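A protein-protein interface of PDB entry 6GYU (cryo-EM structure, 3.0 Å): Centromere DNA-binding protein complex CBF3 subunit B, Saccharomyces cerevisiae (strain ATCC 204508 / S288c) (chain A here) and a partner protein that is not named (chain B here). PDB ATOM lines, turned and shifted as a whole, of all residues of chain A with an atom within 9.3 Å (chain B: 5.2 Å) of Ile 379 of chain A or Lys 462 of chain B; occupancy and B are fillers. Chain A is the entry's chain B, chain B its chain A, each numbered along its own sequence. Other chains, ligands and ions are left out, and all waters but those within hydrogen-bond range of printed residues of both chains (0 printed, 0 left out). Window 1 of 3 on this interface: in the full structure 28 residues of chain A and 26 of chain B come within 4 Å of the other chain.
The side-chain hydroxyl (OG) of Ser 461 of chain B lies within hydrogen-bond range of the side-chain amino group (NZ) of Lys 347 of chain A (3.4 Å).
N of Phe 399 of chain B lies within hydrogen-bond range of OG of Ser 386 of chain A (3.1 Å).
OG of Ser 461 of chain B lies within hydrogen-bond range of NZ of Lys 383 of chain A (3.4 Å).
The side-chain hydroxyl (OG) of Ser 340 of chain A is in hydrogen-bond range of the side-chain amino group (NZ) of Lys 347 of chain A, at 3.3 Å.
Among the printed residues, merely in contact across the chains: Tyr 382 of chain A with Phe 402 of chain B (3.4 Å), Lys 383 of chain A with Phe 399 of chain B (3.5 Å), Arg 375 of chain A with Lys 462 of chain B (3.5 Å), Arg 375 of chain A with Phe 402 of chain B (3.6 Å), Phe 380 of chain A with Ser 461 of chain B (3.8 Å), Ile 379 of chain A with Lys 462 of chain B (3.8 Å), Ile 379 of chain A with Ser 461 of chain B (3.9 Å) and Lys 383 of chain A with Asp 460 of chain B (3.9 Å).
Printed residues of chain B within 4 Å of Arg 375 of chain A: Phe 402 (3.6 Å) and Lys 462 (3.5 Å).
Ile 379 of chain A touches two residues of chain B.
Of the printed residues of chain B, Tyr 382 of chain A touches Phe 402 (3.4 Å).
Of the printed residues of chain A, Phe 399 of chain B touches Lys 383 and Ser 386.
Printed residues of chain A within 4 Å of Phe 402 of chain B: Arg 375 and Tyr 382.
Leu 458 of chain B touches none of the printed residues of chain A.
Ser 461 of chain B touches four residues of chain A.
Lys 462 of chain B touches just these residues of chain A: Arg 375 (3.5 Å) and Ile 379 (3.8 Å).
Arg 463 of chain B touches none of the printed residues of chain A.
The nearest residue of chain B that does not touch Ile 379 of chain A is Phe 399 of chain B (4.1 Å).
The nearest residue of chain A that does not touch Lys 462 of chain B is Lys 383 of chain A (5.2 Å).
The nearest printed residue of chain B that does not touch Phe 380 of chain A is Phe 399 of chain B (6.2 Å).
Hydrophobic or aromatic side chains of chain B within 4 Å of the printed part of chain A: Phe 399 and Phe 402.
Of the 23 printed residues of chain A, 7 touch a printed residue of chain B.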
ATOM      1  N   SER A 317     -24.643   2.880   1.676  1.00  0.00           N
ATOM      2  CA  SER A 317     -23.421   2.896   0.881  1.00  0.00           C
ATOM      3  C   SER A 317     -22.135   2.860   1.696  1.00  0.00           C
ATOM      4  O   SER A 317     -21.054   2.836   1.102  1.00  0.00           O
ATOM      5  CB  SER A 317     -23.391   4.127  -0.032  1.00  0.00           C
ATOM      6  OG  SER A 317     -22.211   4.143  -0.819  1.00  0.00           O
ATOM      7  N   SER A 340     -21.803  -0.303 -12.184  1.00  0.00           N
ATOM      8  CA  SER A 340     -21.782   1.155 -12.070  1.00  0.00           C
ATOM      9  C   SER A 340     -21.970   1.789 -13.441  1.00  0.00           C
ATOM     10  O   SER A 340     -20.998   2.113 -14.128  1.00  0.00           O
ATOM     11  CB  SER A 340     -20.476   1.618 -11.437  1.00  0.00           C
ATOM     12  OG  SER A 340     -20.346   1.127 -10.116  1.00  0.00           O
ATOM     13  N   LEU A 344     -24.271   5.102 -10.276  1.00  0.00           N
ATOM     14  CA  LEU A 344     -23.383   6.220  -9.973  1.00  0.00           C
ATOM     15  C   LEU A 344     -24.174   7.485  -9.662  1.00  0.00           C
ATOM     16  O   LEU A 344     -23.696   8.363  -8.936  1.00  0.00           O
ATOM     17  CB  LEU A 344     -22.427   6.428 -11.153  1.00  0.00           C
ATOM     18  CG  LEU A 344     -21.233   7.391 -11.159  1.00  0.00           C
ATOM     19  CD1 LEU A 344     -21.594   8.811 -11.575  1.00  0.00           C
ATOM     20  CD2 LEU A 344     -20.594   7.400  -9.792  1.00  0.00           C
ATOM     21  N   LYS A 347     -25.443   6.142  -6.070  1.00  0.00           N
ATOM     22  CA  LYS A 347     -24.364   6.065  -5.089  1.00  0.00           C
ATOM     23  C   LYS A 347     -23.880   7.433  -4.635  1.00  0.00           C
ATOM     24  O   LYS A 347     -23.278   7.541  -3.565  1.00  0.00           O
ATOM     25  CB  LYS A 347     -23.179   5.292  -5.655  1.00  0.00           C
ATOM     26  CG  LYS A 347     -23.383   3.810  -5.805  1.00  0.00           C
ATOM     27  CD  LYS A 347     -22.105   3.157  -6.282  1.00  0.00           C
ATOM     28  CE  LYS A 347     -22.259   1.660  -6.397  1.00  0.00           C
ATOM     29  NZ  LYS A 347     -21.003   1.031  -6.873  1.00  0.00           N
ATOM     30  N   ILE A 348     -24.128   8.473  -5.428  1.00  0.00           N
ATOM     31  CA  ILE A 348     -23.790   9.835  -5.049  1.00  0.00           C
ATOM     32  C   ILE A 348     -24.928  10.502  -4.285  1.00  0.00           C
ATOM     33  O   ILE A 348     -24.724  11.570  -3.690  1.00  0.00           O
ATOM     34  CB  ILE A 348     -23.408  10.573  -6.347  1.00  0.00           C
ATOM     35  CG1 ILE A 348     -22.482  11.742  -6.093  1.00  0.00           C
ATOM     36  CG2 ILE A 348     -24.634  11.089  -7.059  1.00  0.00           C
ATOM     37  CD1 ILE A 348     -21.845  12.170  -7.369  1.00  0.00           C
ATOM     38  N   LEU A 351     -24.933   8.583  -0.759  1.00  0.00           N
ATOM     39  CA  LEU A 351     -23.897   9.246   0.009  1.00  0.00           C
ATOM     40  C   LEU A 351     -24.353  10.607   0.517  1.00  0.00           C
ATOM     41  O   LEU A 351     -23.754  11.141   1.455  1.00  0.00           O
ATOM     42  CB  LEU A 351     -22.653   9.380  -0.868  1.00  0.00           C
ATOM     43  CG  LEU A 351     -21.294   9.735  -0.304  1.00  0.00           C
ATOM     44  CD1 LEU A 351     -20.869   8.649   0.650  1.00  0.00           C
ATOM     45  CD2 LEU A 351     -20.334   9.819  -1.459  1.00  0.00           C
ATOM     46  N   ASP A 371     -15.428  10.594   7.622  1.00  0.00           N
ATOM     47  CA  ASP A 371     -14.187  10.258   6.931  1.00  0.00           C
ATOM     48  C   ASP A 371     -14.428   9.229   5.837  1.00  0.00           C
ATOM     49  O   ASP A 371     -13.816   9.300   4.763  1.00  0.00           O
ATOM     50  CB  ASP A 371     -13.153   9.736   7.923  1.00  0.00           C
ATOM     51  CG  ASP A 371     -12.652  10.809   8.865  1.00  0.00           C
ATOM     52  OD1 ASP A 371     -12.687  12.000   8.488  1.00  0.00           O
ATOM     53  OD2 ASP A 371     -12.204  10.458   9.974  1.00  0.00           O
ATOM     54  N   ALA A 372     -15.319   8.263   6.092  1.00  0.00           N
ATOM     55  CA  ALA A 372     -15.680   7.295   5.062  1.00  0.00           C
ATOM     56  C   ALA A 372     -16.375   7.971   3.889  1.00  0.00           C
ATOM     57  O   ALA A 372     -16.087   7.660   2.726  1.00  0.00           O
ATOM     58  CB  ALA A 372     -16.571   6.209   5.658  1.00  0.00           C
ATOM     59  N   ILE A 373     -17.258   8.929   4.177  1.00  0.00           N
ATOM     60  CA  ILE A 373     -17.943   9.683   3.130  1.00  0.00           C
ATOM     61  C   ILE A 373     -16.951  10.525   2.337  1.00  0.00           C
ATOM     62  O   ILE A 373     -17.042  10.607   1.111  1.00  0.00           O
ATOM     63  CB  ILE A 373     -19.076  10.525   3.750  1.00  0.00           C
ATOM     64  CG1 ILE A 373     -20.206   9.613   4.211  1.00  0.00           C
ATOM     65  CG2 ILE A 373     -19.644  11.543   2.781  1.00  0.00           C
ATOM     66  CD1 ILE A 373     -21.230  10.288   5.067  1.00  0.00           C
ATOM     67  N   ARG A 374     -15.940  11.085   3.008  1.00  0.00           N
ATOM     68  CA  ARG A 374     -14.897  11.839   2.314  1.00  0.00           C
ATOM     69  C   ARG A 374     -14.067  10.942   1.394  1.00  0.00           C
ATOM     70  O   ARG A 374     -13.695  11.345   0.278  1.00  0.00           O
ATOM     71  CB  ARG A 374     -14.014  12.529   3.349  1.00  0.00           C
ATOM     72  CG  ARG A 374     -12.996  13.485   2.799  1.00  0.00           C
ATOM     73  CD  ARG A 374     -12.277  14.176   3.939  1.00  0.00           C
ATOM     74  NE  ARG A 374     -11.266  15.111   3.463  1.00  0.00           N
ATOM     75  CZ  ARG A 374     -10.514  15.866   4.256  1.00  0.00           C
ATOM     76  NH1 ARG A 374     -10.658  15.795   5.573  1.00  0.00           N
ATOM     77  NH2 ARG A 374      -9.618  16.693   3.735  1.00  0.00           N
ATOM     78  N   ARG A 375     -13.814   9.703   1.823  1.00  0.00           N
ATOM     79  CA  ARG A 375     -13.101   8.769   0.958  1.00  0.00           C
ATOM     80  C   ARG A 375     -13.937   8.377  -0.258  1.00  0.00           C
ATOM     81  O   ARG A 375     -13.410   8.306  -1.379  1.00  0.00           O
ATOM     82  CB  ARG A 375     -12.669   7.535   1.748  1.00  0.00           C
ATOM     83  CG  ARG A 375     -11.926   6.529   0.894  1.00  0.00           C
ATOM     84  CD  ARG A 375     -10.674   7.153   0.284  1.00  0.00           C
ATOM     85  NE  ARG A 375      -9.988   6.248  -0.634  1.00  0.00           N
ATOM     86  CZ  ARG A 375      -9.035   6.628  -1.477  1.00  0.00           C
ATOM     87  NH1 ARG A 375      -8.461   5.743  -2.281  1.00  0.00           N
ATOM     88  NH2 ARG A 375      -8.660   7.898  -1.527  1.00  0.00           N
ATOM     89  N   GLU A 376     -15.243   8.143  -0.071  1.00  0.00           N
ATOM     90  CA  GLU A 376     -16.073   7.848  -1.239  1.00  0.00           C
ATOM     91  C   GLU A 376     -16.227   9.066  -2.141  1.00  0.00           C
ATOM     92  O   GLU A 376     -16.374   8.913  -3.354  1.00  0.00           O
ATOM     93  CB  GLU A 376     -17.454   7.293  -0.872  1.00  0.00           C
ATOM     94  CG  GLU A 376     -17.470   5.810  -0.525  1.00  0.00           C
ATOM     95  CD  GLU A 376     -17.755   5.525   0.926  1.00  0.00           C
ATOM     96  OE1 GLU A 376     -18.320   6.404   1.599  1.00  0.00           O
ATOM     97  OE2 GLU A 376     -17.393   4.423   1.387  1.00  0.00           O
ATOM     98  N   LEU A 377     -16.174  10.277  -1.577  1.00  0.00           N
ATOM     99  CA  LEU A 377     -16.114  11.488  -2.396  1.00  0.00           C
ATOM    100  C   LEU A 377     -14.897  11.497  -3.304  1.00  0.00           C
ATOM    101  O   LEU A 377     -15.014  11.811  -4.492  1.00  0.00           O
ATOM    102  CB  LEU A 377     -16.105  12.733  -1.519  1.00  0.00           C
ATOM    103  CG  LEU A 377     -17.325  13.611  -1.277  1.00  0.00           C
ATOM    104  CD1 LEU A 377     -18.464  12.909  -0.626  1.00  0.00           C
ATOM    105  CD2 LEU A 377     -16.832  14.698  -0.370  1.00  0.00           C
ATOM    106  N   ASP A 378     -13.729  11.131  -2.768  1.00  0.00           N
ATOM    107  CA  ASP A 378     -12.527  11.064  -3.603  1.00  0.00           C
ATOM    108  C   ASP A 378     -12.644   9.981  -4.679  1.00  0.00           C
ATOM    109  O   ASP A 378     -12.233  10.185  -5.836  1.00  0.00           O
ATOM    110  CB  ASP A 378     -11.299  10.824  -2.728  1.00  0.00           C
ATOM    111  CG  ASP A 378     -10.981  12.007  -1.839  1.00  0.00           C
ATOM    112  OD1 ASP A 378     -11.308  13.147  -2.227  1.00  0.00           O
ATOM    113  OD2 ASP A 378     -10.400  11.797  -0.752  1.00  0.00           O
ATOM    114  N   ILE A 379     -13.247   8.842  -4.320  1.00  0.00           N
ATOM    115  CA  ILE A 379     -13.417   7.745  -5.275  1.00  0.00           C
ATOM    116  C   ILE A 379     -14.375   8.137  -6.399  1.00  0.00           C
ATOM    117  O   ILE A 379     -14.113   7.858  -7.574  1.00  0.00           O
ATOM    118  CB  ILE A 379     -13.874   6.469  -4.543  1.00  0.00           C
ATOM    119  CG1 ILE A 379     -12.775   5.982  -3.601  1.00  0.00           C
ATOM    120  CG2 ILE A 379     -14.219   5.354  -5.513  1.00  0.00           C
ATOM    121  CD1 ILE A 379     -13.220   4.894  -2.660  1.00  0.00           C
ATOM    122  N   PHE A 380     -15.467   8.835  -6.075  1.00  0.00           N
ATOM    123  CA  PHE A 380     -16.405   9.208  -7.130  1.00  0.00           C
ATOM    124  C   PHE A 380     -15.899  10.397  -7.936  1.00  0.00           C
ATOM    125  O   PHE A 380     -16.300  10.575  -9.090  1.00  0.00           O
ATOM    126  CB  PHE A 380     -17.803   9.495  -6.578  1.00  0.00           C
ATOM    127  CG  PHE A 380     -18.483   8.289  -6.006  1.00  0.00           C
ATOM    128  CD1 PHE A 380     -18.674   7.162  -6.783  1.00  0.00           C
ATOM    129  CD2 PHE A 380     -19.032   8.318  -4.739  1.00  0.00           C
ATOM    130  CE1 PHE A 380     -19.307   6.052  -6.270  1.00  0.00           C
ATOM    131  CE2 PHE A 380     -19.666   7.213  -4.219  1.00  0.00           C
ATOM    132  CZ  PHE A 380     -19.803   6.083  -4.986  1.00  0.00           C
ATOM    133  N   GLN A 381     -15.007  11.211  -7.356  1.00  0.00           N
ATOM    134  CA  GLN A 381     -14.285  12.202  -8.152  1.00  0.00           C
ATOM    135  C   GLN A 381     -13.450  11.542  -9.238  1.00  0.00           C
ATOM    136  O   GLN A 381     -13.504  11.946 -10.407  1.00  0.00           O
ATOM    137  CB  GLN A 381     -13.383  13.052  -7.263  1.00  0.00           C
ATOM    138  CG  GLN A 381     -14.043  14.154  -6.464  1.00  0.00           C
ATOM    139  CD  GLN A 381     -14.515  15.300  -7.327  1.00  0.00           C
ATOM    140  OE1 GLN A 381     -13.965  15.550  -8.398  1.00  0.00           O
ATOM    141  NE2 GLN A 381     -15.483  16.052  -6.829  1.00  0.00           N
ATOM    142  N   TYR A 382     -12.680  10.514  -8.876  1.00  0.00           N
ATOM    143  CA  TYR A 382     -11.930   9.801  -9.909  1.00  0.00           C
ATOM    144  C   TYR A 382     -12.834   9.022 -10.855  1.00  0.00           C
ATOM    145  O   TYR A 382     -12.499   8.865 -12.034  1.00  0.00           O
ATOM    146  CB  TYR A 382     -10.894   8.885  -9.278  1.00  0.00           C
ATOM    147  CG  TYR A 382      -9.619   9.606  -8.942  1.00  0.00           C
ATOM    148  CD1 TYR A 382      -8.607   9.723  -9.887  1.00  0.00           C
ATOM    149  CD2 TYR A 382      -9.443  10.218  -7.709  1.00  0.00           C
ATOM    150  CE1 TYR A 382      -7.435  10.379  -9.594  1.00  0.00           C
ATOM    151  CE2 TYR A 382      -8.271  10.888  -7.409  1.00  0.00           C
ATOM    152  CZ  TYR A 382      -7.276  10.963  -8.357  1.00  0.00           C
ATOM    153  OH  TYR A 382      -6.106  11.630  -8.070  1.00  0.00           O
ATOM    154  N   LYS A 383     -13.981   8.550 -10.376  1.00  0.00           N
ATOM    155  CA  LYS A 383     -14.876   7.799 -11.242  1.00  0.00           C
ATOM    156  C   LYS A 383     -15.588   8.692 -12.247  1.00  0.00           C
ATOM    157  O   LYS A 383     -15.842   8.252 -13.372  1.00  0.00           O
ATOM    158  CB  LYS A 383     -15.885   7.026 -10.398  1.00  0.00           C
ATOM    159  CG  LYS A 383     -16.683   5.993 -11.167  1.00  0.00           C
ATOM    160  CD  LYS A 383     -17.625   5.237 -10.255  1.00  0.00           C
ATOM    161  CE  LYS A 383     -17.017   3.928  -9.788  1.00  0.00           C
ATOM    162  NZ  LYS A 383     -16.026   4.129  -8.701  1.00  0.00           N
ATOM    163  N   VAL A 384     -15.894   9.940 -11.886  1.00  0.00           N
ATOM    164  CA  VAL A 384     -16.447  10.871 -12.864  1.00  0.00           C
ATOM    165  C   VAL A 384     -15.344  11.456 -13.744  1.00  0.00           C
ATOM    166  O   VAL A 384     -15.616  11.841 -14.890  1.00  0.00           O
ATOM    167  CB  VAL A 384     -17.285  11.970 -12.170  1.00  0.00           C
ATOM    168  CG1 VAL A 384     -16.426  12.961 -11.409  1.00  0.00           C
ATOM    169  CG2 VAL A 384     -18.191  12.688 -13.153  1.00  0.00           C
ATOM    170  N   ASP A 385     -14.095  11.475 -13.274  1.00  0.00           N
ATOM    171  CA  ASP A 385     -12.989  11.779 -14.173  1.00  0.00           C
ATOM    172  C   ASP A 385     -12.660  10.624 -15.110  1.00  0.00           C
ATOM    173  O   ASP A 385     -11.955  10.832 -16.101  1.00  0.00           O
ATOM    174  CB  ASP A 385     -11.741  12.163 -13.374  1.00  0.00           C
ATOM    175  CG  ASP A 385     -11.890  13.492 -12.668  1.00  0.00           C
ATOM    176  OD1 ASP A 385     -12.673  14.331 -13.154  1.00  0.00           O
ATOM    177  OD2 ASP A 385     -11.223  13.702 -11.631  1.00  0.00           O
ATOM    178  N   SER A 386     -13.152   9.418 -14.822  1.00  0.00           N
ATOM    179  CA  SER A 386     -12.912   8.241 -15.647  1.00  0.00           C
ATOM    180  C   SER A 386     -14.062   7.966 -16.610  1.00  0.00           C
ATOM    181  O   SER A 386     -14.345   6.809 -16.929  1.00  0.00           O
ATOM    182  CB  SER A 386     -12.663   7.019 -14.766  1.00  0.00           C
ATOM    183  OG  SER A 386     -12.474   5.858 -15.554  1.00  0.00           O
ATOM    184  N   ILE A 407     -21.465  15.632  -6.865  1.00  0.00           N
ATOM    185  CA  ILE A 407     -20.352  15.391  -5.953  1.00  0.00           C
ATOM    186  C   ILE A 407     -19.868  16.703  -5.345  1.00  0.00           C
ATOM    187  O   ILE A 407     -19.439  16.727  -4.185  1.00  0.00           O
ATOM    188  CB  ILE A 407     -19.227  14.592  -6.651  1.00  0.00           C
ATOM    189  CG1 ILE A 407     -18.190  14.099  -5.647  1.00  0.00           C
ATOM    190  CG2 ILE A 407     -18.591  15.339  -7.782  1.00  0.00           C
ATOM    191  CD1 ILE A 407     -18.731  13.065  -4.699  1.00  0.00           C
ATOM    192  N   PHE B 399      -9.861   4.601 -14.494  1.00  0.00           N
ATOM    193  CA  PHE B 399     -10.110   4.228 -13.109  1.00  0.00           C
ATOM    194  C   PHE B 399      -9.274   3.031 -12.693  1.00  0.00           C
ATOM    195  O   PHE B 399      -9.008   2.855 -11.499  1.00  0.00           O
ATOM    196  CB  PHE B 399     -11.600   3.940 -12.907  1.00  0.00           C
ATOM    197  CG  PHE B 399     -11.984   3.685 -11.479  1.00  0.00           C
ATOM    198  CD1 PHE B 399     -12.058   4.728 -10.573  1.00  0.00           C
ATOM    199  CD2 PHE B 399     -12.278   2.404 -11.046  1.00  0.00           C
ATOM    200  CE1 PHE B 399     -12.413   4.499  -9.260  1.00  0.00           C
ATOM    201  CE2 PHE B 399     -12.633   2.168  -9.733  1.00  0.00           C
ATOM    202  CZ  PHE B 399     -12.701   3.218  -8.840  1.00  0.00           C
ATOM    203  N   PHE B 402      -6.114   4.550 -11.427  1.00  0.00           N
ATOM    204  CA  PHE B 402      -6.207   5.298 -10.175  1.00  0.00           C
ATOM    205  C   PHE B 402      -5.453   4.604  -9.049  1.00  0.00           C
ATOM    206  O   PHE B 402      -4.448   5.119  -8.551  1.00  0.00           O
ATOM    207  CB  PHE B 402      -7.668   5.517  -9.788  1.00  0.00           C
ATOM    208  CG  PHE B 402      -7.852   5.963  -8.364  1.00  0.00           C
ATOM    209  CD1 PHE B 402      -7.368   7.185  -7.928  1.00  0.00           C
ATOM    210  CD2 PHE B 402      -8.524   5.158  -7.463  1.00  0.00           C
ATOM    211  CE1 PHE B 402      -7.534   7.576  -6.616  1.00  0.00           C
ATOM    212  CE2 PHE B 402      -8.700   5.558  -6.158  1.00  0.00           C
ATOM    213  CZ  PHE B 402      -8.207   6.772  -5.735  1.00  0.00           C
ATOM    214  N   PHE B 403      -5.922   3.434  -8.633  1.00  0.00           N
ATOM    215  CA  PHE B 403      -5.109   2.614  -7.750  1.00  0.00           C
ATOM    216  C   PHE B 403      -4.134   1.824  -8.603  1.00  0.00           C
ATOM    217  O   PHE B 403      -4.536   1.095  -9.513  1.00  0.00           O
ATOM    218  CB  PHE B 403      -5.973   1.719  -6.850  1.00  0.00           C
ATOM    219  CG  PHE B 403      -6.979   0.863  -7.572  1.00  0.00           C
ATOM    220  CD1 PHE B 403      -8.241   1.360  -7.865  1.00  0.00           C
ATOM    221  CD2 PHE B 403      -6.700  -0.459  -7.876  1.00  0.00           C
ATOM    222  CE1 PHE B 403      -9.176   0.581  -8.502  1.00  0.00           C
ATOM    223  CE2 PHE B 403      -7.634  -1.243  -8.514  1.00  0.00           C
ATOM    224  CZ  PHE B 403      -8.876  -0.718  -8.820  1.00  0.00           C
ATOM    225  N   LEU B 458     -17.981  -4.898  -8.714  1.00  0.00           N
ATOM    226  CA  LEU B 458     -17.269  -4.915  -7.453  1.00  0.00           C
ATOM    227  C   LEU B 458     -15.846  -4.402  -7.579  1.00  0.00           C
ATOM    228  O   LEU B 458     -15.278  -3.949  -6.583  1.00  0.00           O
ATOM    229  CB  LEU B 458     -17.266  -6.348  -6.910  1.00  0.00           C
ATOM    230  CG  LEU B 458     -16.836  -6.796  -5.529  1.00  0.00           C
ATOM    231  CD1 LEU B 458     -17.639  -8.020  -5.192  1.00  0.00           C
ATOM    232  CD2 LEU B 458     -15.377  -7.152  -5.522  1.00  0.00           C
ATOM    233  N   PHE B 459     -15.259  -4.476  -8.772  1.00  0.00           N
ATOM    234  CA  PHE B 459     -13.949  -3.886  -9.016  1.00  0.00           C
ATOM    235  C   PHE B 459     -14.010  -2.370  -8.975  1.00  0.00           C
ATOM    236  O   PHE B 459     -13.069  -1.720  -8.508  1.00  0.00           O
ATOM    237  CB  PHE B 459     -13.421  -4.366 -10.361  1.00  0.00           C
ATOM    238  CG  PHE B 459     -12.083  -3.812 -10.729  1.00  0.00           C
ATOM    239  CD1 PHE B 459     -10.932  -4.280 -10.120  1.00  0.00           C
ATOM    240  CD2 PHE B 459     -11.973  -2.844 -11.712  1.00  0.00           C
ATOM    241  CE1 PHE B 459      -9.699  -3.776 -10.471  1.00  0.00           C
ATOM    242  CE2 PHE B 459     -10.746  -2.337 -12.067  1.00  0.00           C
ATOM    243  CZ  PHE B 459      -9.609  -2.807 -11.451  1.00  0.00           C
ATOM    244  N   ASP B 460     -15.102  -1.793  -9.462  1.00  0.00           N
ATOM    245  CA  ASP B 460     -15.313  -0.365  -9.317  1.00  0.00           C
ATOM    246  C   ASP B 460     -15.667  -0.032  -7.870  1.00  0.00           C
ATOM    247  O   ASP B 460     -16.037  -0.903  -7.077  1.00  0.00           O
ATOM    248  CB  ASP B 460     -16.409   0.110 -10.266  1.00  0.00           C
ATOM    249  CG  ASP B 460     -16.011  -0.027 -11.721  1.00  0.00           C
ATOM    250  OD1 ASP B 460     -14.797   0.012 -12.008  1.00  0.00           O
ATOM    251  OD2 ASP B 460     -16.908  -0.171 -12.578  1.00  0.00           O
ATOM    252  N   SER B 461     -15.509   1.252  -7.532  1.00  0.00           N
ATOM    253  CA  SER B 461     -15.680   1.825  -6.191  1.00  0.00           C
ATOM    254  C   SER B 461     -14.730   1.225  -5.154  1.00  0.00           C
ATOM    255  O   SER B 461     -15.007   1.315  -3.952  1.00  0.00           O
ATOM    256  CB  SER B 461     -17.132   1.724  -5.697  1.00  0.00           C
ATOM    257  OG  SER B 461     -17.998   2.508  -6.497  1.00  0.00           O
ATOM    258  N   LYS B 462     -13.609   0.651  -5.615  1.00  0.00           N
ATOM    259  CA  LYS B 462     -12.523   0.118  -4.777  1.00  0.00           C
ATOM    260  C   LYS B 462     -13.011  -0.897  -3.750  1.00  0.00           C
ATOM    261  O   LYS B 462     -12.554  -0.924  -2.607  1.00  0.00           O
ATOM    262  CB  LYS B 462     -11.757   1.237  -4.076  1.00  0.00           C
ATOM    263  CG  LYS B 462     -10.880   2.058  -4.968  1.00  0.00           C
ATOM    264  CD  LYS B 462     -10.179   3.095  -4.131  1.00  0.00           C
ATOM    265  CE  LYS B 462      -9.135   2.460  -3.237  1.00  0.00           C
ATOM    266  NZ  LYS B 462      -8.005   1.909  -4.024  1.00  0.00           N
ATOM    267  N   ARG B 463     -13.957  -1.736  -4.152  1.00  0.00           N
ATOM    268  CA  ARG B 463     -14.511  -2.709  -3.228  1.00  0.00           C
ATOM    269  C   ARG B 463     -13.719  -4.011  -3.223  1.00  0.00           C
ATOM    270  O   ARG B 463     -13.728  -4.724  -2.215  1.00  0.00           O
ATOM    271  CB  ARG B 463     -15.998  -2.917  -3.558  1.00  0.00           C
ATOM    272  CG  ARG B 463     -16.784  -3.833  -2.654  1.00  0.00           C
ATOM    273  CD  ARG B 463     -16.697  -3.442  -1.185  1.00  0.00           C
ATOM    274  NE  ARG B 463     -17.243  -2.129  -0.869  1.00  0.00           N
ATOM    275  CZ  ARG B 463     -17.089  -1.539   0.311  1.00  0.00           C
ATOM    276  NH1 ARG B 463     -17.606  -0.343   0.539  1.00  0.00           N
ATOM    277  NH2 ARG B 463     -16.419  -2.155   1.273  1.00  0.00           N
ATOM    278  N   VAL B 464     -12.978  -4.303  -4.291  1.00  0.00           N
ATOM    279  CA  VAL B 464     -11.827  -5.197  -4.228  1.00  0.00           C
ATOM    280  C   VAL B 464     -10.590  -4.313  -4.149  1.00  0.00           C
ATOM    281  O   VAL B 464     -10.573  -3.202  -4.696  1.00  0.00           O
ATOM    282  CB  VAL B 464     -11.777  -6.172  -5.428  1.00  0.00           C
ATOM    283  CG1 VAL B 464     -11.520  -5.460  -6.729  1.00  0.00           C
ATOM    284  CG2 VAL B 464     -10.737  -7.268  -5.226  1.00  0.00           C
ATOM    285  N   GLU B 465      -9.581  -4.757  -3.401  1.00  0.00           N
ATOM    286  CA  GLU B 465      -8.391  -3.936  -3.194  1.00  0.00           C
ATOM    287  C   GLU B 465      -7.174  -4.824  -2.931  1.00  0.00           C
ATOM    288  O   GLU B 465      -6.916  -5.233  -1.797  1.00  0.00           O
ATOM    289  CB  GLU B 465      -8.646  -2.920  -2.086  1.00  0.00           C
ATOM    290  CG  GLU B 465      -9.393  -3.457  -0.875  1.00  0.00           C
ATOM    291  CD  GLU B 465      -9.788  -2.378   0.093  1.00  0.00           C
ATOM    292  OE1 GLU B 465      -9.471  -1.200  -0.177  1.00  0.00           O
ATOM    293  OE2 GLU B 465     -10.407  -2.691   1.127  1.00  0.00           O
